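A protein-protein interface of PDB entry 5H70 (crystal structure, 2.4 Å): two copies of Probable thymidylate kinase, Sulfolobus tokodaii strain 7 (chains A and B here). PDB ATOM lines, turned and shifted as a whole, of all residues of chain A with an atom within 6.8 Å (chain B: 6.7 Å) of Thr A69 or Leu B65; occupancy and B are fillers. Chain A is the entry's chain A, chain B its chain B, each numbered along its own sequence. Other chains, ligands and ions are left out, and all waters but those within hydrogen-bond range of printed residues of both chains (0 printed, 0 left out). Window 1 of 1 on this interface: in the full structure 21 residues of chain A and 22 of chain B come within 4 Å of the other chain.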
ATOM      1  N   ILE A  45     -15.108  10.749  -5.694  1.00  0.00           N
ATOM      2  CA  ILE A  45     -14.802   9.346  -5.445  1.00  0.00           C
ATOM      3  C   ILE A  45     -14.500   8.622  -6.752  1.00  0.00           C
ATOM      4  O   ILE A  45     -13.575   7.801  -6.822  1.00  0.00           O
ATOM      5  CB  ILE A  45     -15.947   8.681  -4.669  1.00  0.00           C
ATOM      6  CG1 ILE A  45     -15.991   9.259  -3.260  1.00  0.00           C
ATOM      7  CG2 ILE A  45     -15.738   7.188  -4.621  1.00  0.00           C
ATOM      8  CD1 ILE A  45     -17.063   8.703  -2.401  1.00  0.00           C
ATOM      9  N   HIS A  46     -15.267   8.912  -7.805  1.00  0.00           N
ATOM     10  CA  HIS A  46     -14.937   8.390  -9.125  1.00  0.00           C
ATOM     11  C   HIS A  46     -13.536   8.823  -9.552  1.00  0.00           C
ATOM     12  O   HIS A  46     -12.814   8.046 -10.189  1.00  0.00           O
ATOM     13  CB  HIS A  46     -16.013   8.836 -10.128  1.00  0.00           C
ATOM     14  CG  HIS A  46     -15.543   8.960 -11.550  1.00  0.00           C
ATOM     15  ND1 HIS A  46     -15.139  10.160 -12.101  1.00  0.00           N
ATOM     16  CD2 HIS A  46     -15.450   8.043 -12.544  1.00  0.00           C
ATOM     17  CE1 HIS A  46     -14.803   9.974 -13.365  1.00  0.00           C
ATOM     18  NE2 HIS A  46     -14.982   8.699 -13.660  1.00  0.00           N
ATOM     19  N   ILE A  49     -10.636   6.748  -7.621  1.00  0.00           N
ATOM     20  CA  ILE A  49     -10.538   5.348  -8.014  1.00  0.00           C
ATOM     21  C   ILE A  49     -10.058   5.220  -9.458  1.00  0.00           C
ATOM     22  O   ILE A  49      -9.224   4.362  -9.768  1.00  0.00           O
ATOM     23  CB  ILE A  49     -11.879   4.618  -7.784  1.00  0.00           C
ATOM     24  CG1 ILE A  49     -12.238   4.607  -6.293  1.00  0.00           C
ATOM     25  CG2 ILE A  49     -11.830   3.182  -8.320  1.00  0.00           C
ATOM     26  CD1 ILE A  49     -13.668   3.989  -5.976  1.00  0.00           C
ATOM     27  N   SER A  64     -19.557  -0.093 -12.874  1.00  0.00           N
ATOM     28  CA  SER A  64     -20.911   0.166 -12.403  1.00  0.00           C
ATOM     29  C   SER A  64     -20.937   0.442 -10.901  1.00  0.00           C
ATOM     30  O   SER A  64     -21.610   1.373 -10.438  1.00  0.00           O
ATOM     31  CB  SER A  64     -21.793  -1.018 -12.785  1.00  0.00           C
ATOM     32  OG  SER A  64     -22.946  -1.101 -11.997  1.00  0.00           O
ATOM     33  N   LEU A  65     -20.189  -0.334 -10.118  1.00  0.00           N
ATOM     34  CA  LEU A  65     -20.156  -0.050  -8.691  1.00  0.00           C
ATOM     35  C   LEU A  65     -19.455   1.264  -8.380  1.00  0.00           C
ATOM     36  O   LEU A  65     -19.815   1.942  -7.405  1.00  0.00           O
ATOM     37  CB  LEU A  65     -19.507  -1.204  -7.924  1.00  0.00           C
ATOM     38  CG  LEU A  65     -20.335  -2.482  -7.963  1.00  0.00           C
ATOM     39  CD1 LEU A  65     -19.527  -3.639  -7.458  1.00  0.00           C
ATOM     40  CD2 LEU A  65     -21.581  -2.290  -7.093  1.00  0.00           C
ATOM     41  N   ILE A  66     -18.461   1.653  -9.178  1.00  0.00           N
ATOM     42  CA  ILE A  66     -17.786   2.924  -8.920  1.00  0.00           C
ATOM     43  C   ILE A  66     -18.754   4.091  -9.100  1.00  0.00           C
ATOM     44  O   ILE A  66     -18.792   5.026  -8.288  1.00  0.00           O
ATOM     45  CB  ILE A  66     -16.562   3.078  -9.829  1.00  0.00           C
ATOM     46  CG1 ILE A  66     -15.468   2.082  -9.433  1.00  0.00           C
ATOM     47  CG2 ILE A  66     -16.037   4.503  -9.729  1.00  0.00           C
ATOM     48  CD1 ILE A  66     -14.515   1.844 -10.555  1.00  0.00           C
ATOM     49  N   HIS A  67     -19.553   4.060 -10.163  1.00  0.00           N
ATOM     50  CA  HIS A  67     -20.420   5.203 -10.408  1.00  0.00           C
ATOM     51  C   HIS A  67     -21.514   5.281  -9.352  1.00  0.00           C
ATOM     52  O   HIS A  67     -21.709   6.333  -8.744  1.00  0.00           O
ATOM     53  CB  HIS A  67     -21.022   5.103 -11.808  1.00  0.00           C
ATOM     54  CG  HIS A  67     -20.030   5.301 -12.908  1.00  0.00           C
ATOM     55  ND1 HIS A  67     -19.937   4.451 -13.991  1.00  0.00           N
ATOM     56  CD2 HIS A  67     -19.114   6.274 -13.116  1.00  0.00           C
ATOM     57  CE1 HIS A  67     -18.992   4.879 -14.806  1.00  0.00           C
ATOM     58  NE2 HIS A  67     -18.475   5.984 -14.298  1.00  0.00           N
ATOM     59  N   ALA A  68     -22.086   4.128  -8.990  1.00  0.00           N
ATOM     60  CA  ALA A  68     -23.128   4.092  -7.982  1.00  0.00           C
ATOM     61  C   ALA A  68     -22.592   4.551  -6.641  1.00  0.00           C
ATOM     62  O   ALA A  68     -23.266   5.294  -5.925  1.00  0.00           O
ATOM     63  CB  ALA A  68     -23.711   2.678  -7.899  1.00  0.00           C
ATOM     64  N   THR A  69     -21.354   4.171  -6.319  1.00  0.00           N
ATOM     65  CA  THR A  69     -20.729   4.649  -5.092  1.00  0.00           C
ATOM     66  C   THR A  69     -20.657   6.156  -5.076  1.00  0.00           C
ATOM     67  O   THR A  69     -21.004   6.798  -4.080  1.00  0.00           O
ATOM     68  CB  THR A  69     -19.324   4.064  -4.957  1.00  0.00           C
ATOM     69  OG1 THR A  69     -19.399   2.630  -5.009  1.00  0.00           O
ATOM     70  CG2 THR A  69     -18.623   4.563  -3.696  1.00  0.00           C
ATOM     71  N   ASP A  70     -20.204   6.735  -6.181  1.00  0.00           N
ATOM     72  CA  ASP A  70     -20.027   8.172  -6.218  1.00  0.00           C
ATOM     73  C   ASP A  70     -21.389   8.865  -6.219  1.00  0.00           C
ATOM     74  O   ASP A  70     -21.585   9.871  -5.535  1.00  0.00           O
ATOM     75  CB  ASP A  70     -19.195   8.540  -7.442  1.00  0.00           C
ATOM     76  CG  ASP A  70     -18.943   9.997  -7.527  1.00  0.00           C
ATOM     77  OD1 ASP A  70     -19.583  10.656  -8.366  1.00  0.00           O
ATOM     78  OD2 ASP A  70     -18.115  10.482  -6.731  1.00  0.00           O
ATOM     79  N   PHE A  71     -22.368   8.274  -6.896  1.00  0.00           N
ATOM     80  CA  PHE A  71     -23.710   8.821  -6.845  1.00  0.00           C
ATOM     81  C   PHE A  71     -24.309   8.719  -5.443  1.00  0.00           C
ATOM     82  O   PHE A  71     -24.963   9.661  -4.972  1.00  0.00           O
ATOM     83  CB  PHE A  71     -24.604   8.114  -7.853  1.00  0.00           C
ATOM     84  CG  PHE A  71     -26.064   8.365  -7.627  1.00  0.00           C
ATOM     85  CD1 PHE A  71     -26.669   9.470  -8.208  1.00  0.00           C
ATOM     86  CD2 PHE A  71     -26.846   7.483  -6.907  1.00  0.00           C
ATOM     87  CE1 PHE A  71     -28.017   9.730  -8.023  1.00  0.00           C
ATOM     88  CE2 PHE A  71     -28.199   7.721  -6.731  1.00  0.00           C
ATOM     89  CZ  PHE A  71     -28.789   8.856  -7.289  1.00  0.00           C
ATOM     90  N   SER A  72     -24.084   7.605  -4.747  1.00  0.00           N
ATOM     91  CA  SER A  72     -24.656   7.483  -3.412  1.00  0.00           C
ATOM     92  C   SER A  72     -24.167   8.606  -2.509  1.00  0.00           C
ATOM     93  O   SER A  72     -24.897   9.041  -1.611  1.00  0.00           O
ATOM     94  CB  SER A  72     -24.357   6.118  -2.782  1.00  0.00           C
ATOM     95  OG  SER A  72     -23.084   6.106  -2.173  1.00  0.00           O
ATOM     96  N   ASP A  73     -22.939   9.085  -2.705  1.00  0.00           N
ATOM     97  CA  ASP A  73     -22.463  10.137  -1.815  1.00  0.00           C
ATOM     98  C   ASP A  73     -23.138  11.471  -2.162  1.00  0.00           C
ATOM     99  O   ASP A  73     -23.519  12.227  -1.272  1.00  0.00           O
ATOM    100  CB  ASP A  73     -20.937  10.239  -1.899  1.00  0.00           C
ATOM    101  CG  ASP A  73     -20.388  11.492  -1.253  1.00  0.00           C
ATOM    102  OD1 ASP A  73     -20.819  11.795  -0.126  1.00  0.00           O
ATOM    103  OD2 ASP A  73     -19.554  12.186  -1.879  1.00  0.00           O
ATOM    104  N   ARG A  74     -23.333  11.762  -3.450  1.00  0.00           N
ATOM    105  CA  ARG A  74     -24.030  12.993  -3.802  1.00  0.00           C
ATOM    106  C   ARG A  74     -25.486  12.913  -3.392  1.00  0.00           C
ATOM    107  O   ARG A  74     -26.062  13.908  -2.948  1.00  0.00           O
ATOM    108  CB  ARG A  74     -23.907  13.287  -5.298  1.00  0.00           C
ATOM    109  CG  ARG A  74     -22.505  13.710  -5.724  1.00  0.00           C
ATOM    110  CD  ARG A  74     -22.505  14.408  -7.083  1.00  0.00           C
ATOM    111  NE  ARG A  74     -23.061  13.550  -8.127  1.00  0.00           N
ATOM    112  CZ  ARG A  74     -22.423  12.511  -8.659  1.00  0.00           C
ATOM    113  NH1 ARG A  74     -21.205  12.199  -8.244  1.00  0.00           N
ATOM    114  NH2 ARG A  74     -23.005  11.778  -9.601  1.00  0.00           N
ATOM    115  N   LEU A 115     -29.461  -2.202  -7.230  1.00  0.00           N
ATOM    116  CA  LEU A 115     -28.332  -1.410  -6.762  1.00  0.00           C
ATOM    117  C   LEU A 115     -28.777   0.013  -6.409  1.00  0.00           C
ATOM    118  O   LEU A 115     -28.411   0.543  -5.357  1.00  0.00           O
ATOM    119  CB  LEU A 115     -27.231  -1.413  -7.831  1.00  0.00           C
ATOM    120  CG  LEU A 115     -25.987  -0.513  -7.774  1.00  0.00           C
ATOM    121  CD1 LEU A 115     -25.195  -0.706  -6.513  1.00  0.00           C
ATOM    122  CD2 LEU A 115     -25.085  -0.759  -8.979  1.00  0.00           C
ATOM    123  N   TYR A 116     -29.589   0.635  -7.264  1.00  0.00           N
ATOM    124  CA  TYR A 116     -29.998   2.020  -7.071  1.00  0.00           C
ATOM    125  C   TYR A 116     -31.325   2.205  -6.321  1.00  0.00           C
ATOM    126  O   TYR A 116     -31.775   3.347  -6.168  1.00  0.00           O
ATOM    127  CB  TYR A 116     -30.079   2.717  -8.426  1.00  0.00           C
ATOM    128  CG  TYR A 116     -28.728   3.098  -8.971  1.00  0.00           C
ATOM    129  CD1 TYR A 116     -28.135   4.288  -8.587  1.00  0.00           C
ATOM    130  CD2 TYR A 116     -28.040   2.265  -9.870  1.00  0.00           C
ATOM    131  CE1 TYR A 116     -26.919   4.682  -9.080  1.00  0.00           C
ATOM    132  CE2 TYR A 116     -26.794   2.643 -10.376  1.00  0.00           C
ATOM    133  CZ  TYR A 116     -26.247   3.871  -9.971  1.00  0.00           C
ATOM    134  OH  TYR A 116     -25.026   4.311 -10.419  1.00  0.00           O
ATOM    135  N   PHE A 118     -31.951   2.395  -3.392  1.00  0.00           N
ATOM    136  CA  PHE A 118     -31.855   3.342  -2.294  1.00  0.00           C
ATOM    137  C   PHE A 118     -32.258   4.757  -2.715  1.00  0.00           C
ATOM    138  O   PHE A 118     -32.348   5.637  -1.852  1.00  0.00           O
ATOM    139  CB  PHE A 118     -30.429   3.357  -1.723  1.00  0.00           C
ATOM    140  CG  PHE A 118     -29.383   3.875  -2.683  1.00  0.00           C
ATOM    141  CD1 PHE A 118     -29.204   5.264  -2.875  1.00  0.00           C
ATOM    142  CD2 PHE A 118     -28.561   3.003  -3.368  1.00  0.00           C
ATOM    143  CE1 PHE A 118     -28.254   5.761  -3.759  1.00  0.00           C
ATOM    144  CE2 PHE A 118     -27.578   3.477  -4.244  1.00  0.00           C
ATOM    145  CZ  PHE A 118     -27.412   4.850  -4.443  1.00  0.00           C
ATOM    146  N   TRP B  44      -6.657   2.883  -2.407  1.00  0.00           N
ATOM    147  CA  TRP B  44      -7.571   3.960  -2.774  1.00  0.00           C
ATOM    148  C   TRP B  44      -8.732   4.097  -1.785  1.00  0.00           C
ATOM    149  O   TRP B  44      -9.361   5.157  -1.741  1.00  0.00           O
ATOM    150  CB  TRP B  44      -8.103   3.782  -4.212  1.00  0.00           C
ATOM    151  CG  TRP B  44      -8.821   2.475  -4.530  1.00  0.00           C
ATOM    152  CD1 TRP B  44      -8.313   1.406  -5.218  1.00  0.00           C
ATOM    153  CD2 TRP B  44     -10.180   2.120  -4.190  1.00  0.00           C
ATOM    154  NE1 TRP B  44      -9.264   0.409  -5.319  1.00  0.00           N
ATOM    155  CE2 TRP B  44     -10.416   0.826  -4.702  1.00  0.00           C
ATOM    156  CE3 TRP B  44     -11.213   2.770  -3.501  1.00  0.00           C
ATOM    157  CZ2 TRP B  44     -11.650   0.170  -4.546  1.00  0.00           C
ATOM    158  CZ3 TRP B  44     -12.440   2.121  -3.350  1.00  0.00           C
ATOM    159  CH2 TRP B  44     -12.643   0.830  -3.861  1.00  0.00           C
ATOM    160  N   PRO B  60     -22.955   5.004   5.959  1.00  0.00           N
ATOM    161  CA  PRO B  60     -22.725   3.547   5.848  1.00  0.00           C
ATOM    162  C   PRO B  60     -23.034   3.013   4.457  1.00  0.00           C
ATOM    163  O   PRO B  60     -22.363   2.080   3.998  1.00  0.00           O
ATOM    164  CB  PRO B  60     -23.661   2.939   6.907  1.00  0.00           C
ATOM    165  CG  PRO B  60     -23.989   4.074   7.887  1.00  0.00           C
ATOM    166  CD  PRO B  60     -23.598   5.398   7.236  1.00  0.00           C
ATOM    167  N   LEU B  61     -24.059   3.555   3.789  1.00  0.00           N
ATOM    168  CA  LEU B  61     -24.378   3.138   2.426  1.00  0.00           C
ATOM    169  C   LEU B  61     -23.188   3.321   1.474  1.00  0.00           C
ATOM    170  O   LEU B  61     -22.835   2.407   0.728  1.00  0.00           O
ATOM    171  CB  LEU B  61     -25.596   3.895   1.918  1.00  0.00           C
ATOM    172  CG  LEU B  61     -25.775   3.764   0.408  1.00  0.00           C
ATOM    173  CD1 LEU B  61     -26.073   2.320   0.049  1.00  0.00           C
ATOM    174  CD2 LEU B  61     -26.895   4.654  -0.093  1.00  0.00           C
ATOM    175  N   THR B  62     -22.562   4.496   1.481  1.00  0.00           N
ATOM    176  CA  THR B  62     -21.444   4.713   0.571  1.00  0.00           C
ATOM    177  C   THR B  62     -20.266   3.800   0.905  1.00  0.00           C
ATOM    178  O   THR B  62     -19.645   3.236   0.001  1.00  0.00           O
ATOM    179  CB  THR B  62     -21.056   6.194   0.599  1.00  0.00           C
ATOM    180  OG1 THR B  62     -22.116   6.922  -0.029  1.00  0.00           O
ATOM    181  CG2 THR B  62     -19.756   6.478  -0.161  1.00  0.00           C
ATOM    182  N   PHE B  63     -19.992   3.604   2.204  1.00  0.00           N
ATOM    183  CA  PHE B  63     -18.979   2.655   2.655  1.00  0.00           C
ATOM    184  C   PHE B  63     -19.284   1.251   2.182  1.00  0.00           C
ATOM    185  O   PHE B  63     -18.391   0.546   1.701  1.00  0.00           O
ATOM    186  CB  PHE B  63     -18.852   2.683   4.173  1.00  0.00           C
ATOM    187  CG  PHE B  63     -17.794   3.615   4.658  1.00  0.00           C
ATOM    188  CD1 PHE B  63     -16.453   3.300   4.489  1.00  0.00           C
ATOM    189  CD2 PHE B  63     -18.133   4.827   5.258  1.00  0.00           C
ATOM    190  CE1 PHE B  63     -15.461   4.173   4.927  1.00  0.00           C
ATOM    191  CE2 PHE B  63     -17.146   5.706   5.699  1.00  0.00           C
ATOM    192  CZ  PHE B  63     -15.806   5.383   5.532  1.00  0.00           C
ATOM    193  N   SER B  64     -20.544   0.845   2.260  1.00  0.00           N
ATOM    194  CA  SER B  64     -20.909  -0.454   1.718  1.00  0.00           C
ATOM    195  C   SER B  64     -20.627  -0.501   0.216  1.00  0.00           C
ATOM    196  O   SER B  64     -20.010  -1.451  -0.281  1.00  0.00           O
ATOM    197  CB  SER B  64     -22.377  -0.728   2.027  1.00  0.00           C
ATOM    198  OG  SER B  64     -22.923  -1.600   1.088  1.00  0.00           O
ATOM    199  N   LEU B  65     -20.988   0.550  -0.524  1.00  0.00           N
ATOM    200  CA  LEU B  65     -20.664   0.492  -1.945  1.00  0.00           C
ATOM    201  C   LEU B  65     -19.159   0.525  -2.201  1.00  0.00           C
ATOM    202  O   LEU B  65     -18.700  -0.074  -3.175  1.00  0.00           O
ATOM    203  CB  LEU B  65     -21.365   1.588  -2.748  1.00  0.00           C
ATOM    204  CG  LEU B  65     -22.877   1.402  -2.787  1.00  0.00           C
ATOM    205  CD1 LEU B  65     -23.634   2.643  -3.148  1.00  0.00           C
ATOM    206  CD2 LEU B  65     -23.105   0.314  -3.815  1.00  0.00           C
ATOM    207  N   ILE B  66     -18.388   1.200  -1.345  1.00  0.00           N
ATOM    208  CA  ILE B  66     -16.942   1.230  -1.513  1.00  0.00           C
ATOM    209  C   ILE B  66     -16.364  -0.177  -1.385  1.00  0.00           C
ATOM    210  O   ILE B  66     -15.584  -0.626  -2.239  1.00  0.00           O
ATOM    211  CB  ILE B  66     -16.309   2.193  -0.499  1.00  0.00           C
ATOM    212  CG1 ILE B  66     -16.632   3.648  -0.878  1.00  0.00           C
ATOM    213  CG2 ILE B  66     -14.827   1.942  -0.423  1.00  0.00           C
ATOM    214  CD1 ILE B  66     -16.455   4.649   0.253  1.00  0.00           C
ATOM    215  N   HIS B  67     -16.803  -0.926  -0.364  1.00  0.00           N
ATOM    216  CA  HIS B  67     -16.228  -2.247  -0.165  1.00  0.00           C
ATOM    217  C   HIS B  67     -16.673  -3.202  -1.248  1.00  0.00           C
ATOM    218  O   HIS B  67     -15.876  -4.015  -1.714  1.00  0.00           O
ATOM    219  CB  HIS B  67     -16.563  -2.788   1.221  1.00  0.00           C
ATOM    220  CG  HIS B  67     -15.926  -1.999   2.319  1.00  0.00           C
ATOM    221  ND1 HIS B  67     -14.561  -1.989   2.513  1.00  0.00           N
ATOM    222  CD2 HIS B  67     -16.448  -1.233   3.301  1.00  0.00           C
ATOM    223  CE1 HIS B  67     -14.265  -1.210   3.534  1.00  0.00           C
ATOM    224  NE2 HIS B  67     -15.393  -0.748   4.038  1.00  0.00           N
ATOM    225  N   ALA B  68     -17.923  -3.096  -1.698  1.00  0.00           N
ATOM    226  CA  ALA B  68     -18.356  -3.960  -2.791  1.00  0.00           C
ATOM    227  C   ALA B  68     -17.584  -3.661  -4.072  1.00  0.00           C
ATOM    228  O   ALA B  68     -17.257  -4.579  -4.832  1.00  0.00           O
ATOM    229  CB  ALA B  68     -19.853  -3.805  -3.016  1.00  0.00           C
ATOM    230  N   THR B  69     -17.290  -2.379  -4.333  1.00  0.00           N
ATOM    231  CA  THR B  69     -16.447  -2.035  -5.474  1.00  0.00           C
ATOM    232  C   THR B  69     -15.080  -2.685  -5.361  1.00  0.00           C
ATOM    233  O   THR B  69     -14.565  -3.253  -6.331  1.00  0.00           O
ATOM    234  CB  THR B  69     -16.279  -0.518  -5.592  1.00  0.00           C
ATOM    235  OG1 THR B  69     -17.553   0.124  -5.677  1.00  0.00           O
ATOM    236  CG2 THR B  69     -15.401  -0.158  -6.760  1.00  0.00           C
ATOM    237  N   ASP B  70     -14.490  -2.612  -4.174  1.00  0.00           N
ATOM    238  CA  ASP B  70     -13.142  -3.102  -3.952  1.00  0.00           C
ATOM    239  C   ASP B  70     -13.116  -4.620  -4.081  1.00  0.00           C
ATOM    240  O   ASP B  70     -12.191  -5.190  -4.677  1.00  0.00           O
ATOM    241  CB  ASP B  70     -12.695  -2.612  -2.570  1.00  0.00           C
ATOM    242  CG  ASP B  70     -11.283  -3.005  -2.209  1.00  0.00           C
ATOM    243  OD1 ASP B  70     -10.404  -3.049  -3.096  1.00  0.00           O
ATOM    244  OD2 ASP B  70     -11.050  -3.254  -1.008  1.00  0.00           O
ATOM    245  N   ASP B 102     -22.341  -4.321   7.205  1.00  0.00           N
ATOM    246  CA  ASP B 102     -23.194  -3.290   6.676  1.00  0.00           C
ATOM    247  C   ASP B 102     -24.567  -3.289   7.329  1.00  0.00           C
ATOM    248  O   ASP B 102     -25.116  -2.214   7.602  1.00  0.00           O
ATOM    249  CB  ASP B 102     -23.325  -3.420   5.150  1.00  0.00           C
ATOM    250  CG  ASP B 102     -21.974  -3.246   4.417  1.00  0.00           C
ATOM    251  OD1 ASP B 102     -21.132  -2.456   4.891  1.00  0.00           O
ATOM    252  OD2 ASP B 102     -21.768  -3.860   3.349  1.00  0.00           O
ATOM    253  N   TRP B 111     -30.790  -5.813   0.870  1.00  0.00           N
ATOM    254  CA  TRP B 111     -30.242  -5.082  -0.266  1.00  0.00           C
ATOM    255  C   TRP B 111     -28.768  -5.423  -0.497  1.00  0.00           C
ATOM    256  O   TRP B 111     -28.319  -5.505  -1.643  1.00  0.00           O
ATOM    257  CB  TRP B 111     -30.441  -3.596  -0.048  1.00  0.00           C
ATOM    258  CG  TRP B 111     -29.793  -2.736  -1.044  1.00  0.00           C
ATOM    259  CD1 TRP B 111     -30.335  -2.273  -2.212  1.00  0.00           C
ATOM    260  CD2 TRP B 111     -28.486  -2.182  -0.961  1.00  0.00           C
ATOM    261  NE1 TRP B 111     -29.435  -1.472  -2.863  1.00  0.00           N
ATOM    262  CE2 TRP B 111     -28.292  -1.392  -2.111  1.00  0.00           C
ATOM    263  CE3 TRP B 111     -27.454  -2.280  -0.027  1.00  0.00           C
ATOM    264  CZ2 TRP B 111     -27.097  -0.712  -2.355  1.00  0.00           C
ATOM    265  CZ3 TRP B 111     -26.268  -1.607  -0.265  1.00  0.00           C
ATOM    266  CH2 TRP B 111     -26.100  -0.830  -1.417  1.00  0.00           C
ATOM    267  N   LEU B 115     -26.754  -6.803  -3.697  1.00  0.00           N
ATOM    268  CA  LEU B 115     -25.546  -6.142  -4.181  1.00  0.00           C
ATOM    269  C   LEU B 115     -24.438  -7.153  -4.521  1.00  0.00           C
ATOM    270  O   LEU B 115     -23.864  -7.120  -5.616  1.00  0.00           O
ATOM    271  CB  LEU B 115     -25.088  -5.140  -3.124  1.00  0.00           C
ATOM    272  CG  LEU B 115     -23.713  -4.497  -3.213  1.00  0.00           C
ATOM    273  CD1 LEU B 115     -23.639  -3.636  -4.458  1.00  0.00           C
ATOM    274  CD2 LEU B 115     -23.425  -3.683  -1.957  1.00  0.00           C
ATOM    275  N   TYR B 116     -24.171  -8.097  -3.612  1.00  0.00           N
ATOM    276  CA  TYR B 116     -23.120  -9.090  -3.770  1.00  0.00           C
ATOM    277  C   TYR B 116     -23.587 -10.324  -4.520  1.00  0.00           C
ATOM    278  O   TYR B 116     -22.847 -11.317  -4.579  1.00  0.00           O
ATOM    279  CB  TYR B 116     -22.575  -9.514  -2.408  1.00  0.00           C
ATOM    280  CG  TYR B 116     -21.633  -8.510  -1.820  1.00  0.00           C
ATOM    281  CD1 TYR B 116     -20.304  -8.520  -2.165  1.00  0.00           C
ATOM    282  CD2 TYR B 116     -22.065  -7.529  -0.946  1.00  0.00           C
ATOM    283  CE1 TYR B 116     -19.426  -7.625  -1.654  1.00  0.00           C
ATOM    284  CE2 TYR B 116     -21.170  -6.601  -0.422  1.00  0.00           C
ATOM    285  CZ  TYR B 116     -19.838  -6.667  -0.783  1.00  0.00           C
ATOM    286  OH  TYR B 116     -18.892  -5.775  -0.301  1.00  0.00           O
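The side-chain hydroxyl (OG) of Ser A72 sits at hydrogen-bond distance from the side-chain hydroxyl (OG1) of Thr B62, 2.5 Å away.
The side-chain hydroxyl (OG1) of Thr B69 lies close to the backbone carbonyl oxygen (O) of Leu A65, at 3.4 Å.
O of Leu A115 is in hydrogen-bond range of NE1 of Trp B111 (3.4 Å).
OG1 of Thr B69 sits at hydrogen-bond distance from OG1 of Thr A69 (3.2 Å).
O of Leu B65 sits close to OG1 of Thr A69, 3.3 Å away.
The backbone carbonyl oxygen (O) of Leu A65 sits at hydrogen-bond distance from the side-chain hydroxyl (OG1) of Thr A69, 2.5 Å away.
The backbone carbonyl oxygen of Thr A69 is in hydrogen-bond range of the side-chain hydroxyl of Ser A72 (2.9 Å).
N of Ala A68 sits close to OH of Tyr A116 (3.3 Å).
The backbone NH (N) of Ala B68 lies close to the side-chain hydroxyl (OH) of Tyr B116.
The side-chain hydroxyl (OG1) of Thr B69 lies within hydrogen-bond range of the backbone carbonyl oxygen (O) of Leu B65 (2.8 Å).
Among the printed residues, merely in contact across the chains: Ile A49 with Trp B44 (3.4 Å), Ile A66 with Thr B69 (3.5 Å), Asp A73 with Thr B62 (3.5 Å), Leu A115 with Leu B65 (3.6 Å), Ser A72 with Leu B65 (3.6 Å), Thr A69 with Ile B66 (3.6 Å), Leu A65 with Ala B68 (3.6 Å), Leu A65 with Leu B115 (3.6 Å), Phe A118 with Leu B61 (3.7 Å), Ala A68 with Leu B65 (3.9 Å), Leu A115 with Leu B115 (3.9 Å) and Ser A72 with Leu B61 (3.98 Å).
Ile A45 touches none of the printed residues of chain B.
Of the printed residues of chain B, Ala A68 touches Leu B65.
Of the printed residues of chain B, Thr A69 touches Leu B65, Ile B66 and Thr B69.
Of the printed residues of chain B, Ser A72 touches Leu B61, Thr B62 and Leu B65.
Of the printed residues of chain B, Asp A73 touches Thr B62.
Of chain A, only Ala A68, Thr A69, Ser A72 and Leu A115 come within 4 Å of Leu B65.
Asp B70 touches none of the printed residues of chain A.
The nearest residue of chain A that does not touch Leu B65 is Phe A118 (4.2 Å).
The nearest printed residue of chain A that does not touch Trp B111 is Phe A118 (4.1 Å).
Hydrophobic or aromatic side chains of chain B that line the printed part of chain A: Trp B44, Leu B61, Leu B65, Ile B66, Trp B111 and Leu B115.
Of the 17 printed residues of chain A, 9 touch a printed residue of chain B.
Printed residues of chain A that touch a printed residue of chain B: Ile A49, Leu A65, Ile A66, Ala A68, Thr A69, Ser A72, Asp A73, Leu A115 and Phe A118.
Hydrophobic or aromatic side chains of chain A that line the printed part of chain B: Ile A49, Leu A65, Ile A66, Leu A115 and Phe A118.
Among the printed residues, 17 pairs touch across the chains.
Among the printed residues, no Asp or Glu carboxylate lies within 4 Å of a Lys or Arg side-chain nitrogen of the other chain.
Leu A65 touches Thr B69, and with the chains exchanged Thr A69 touches Leu B65.
Leu A65 touches Leu B115, and with the chains exchanged Leu A115 touches Leu B65.
Ile A66 touches Thr B69, and with the chains exchanged Thr A69 touches Ile B66.
Leu A115 touches its own counterpart, Leu B115.
9 positions are printed for both chains.
Of the 17 pairs that touch across the chains among the printed residues, 10 have their exchanged pair printed and touching as well.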
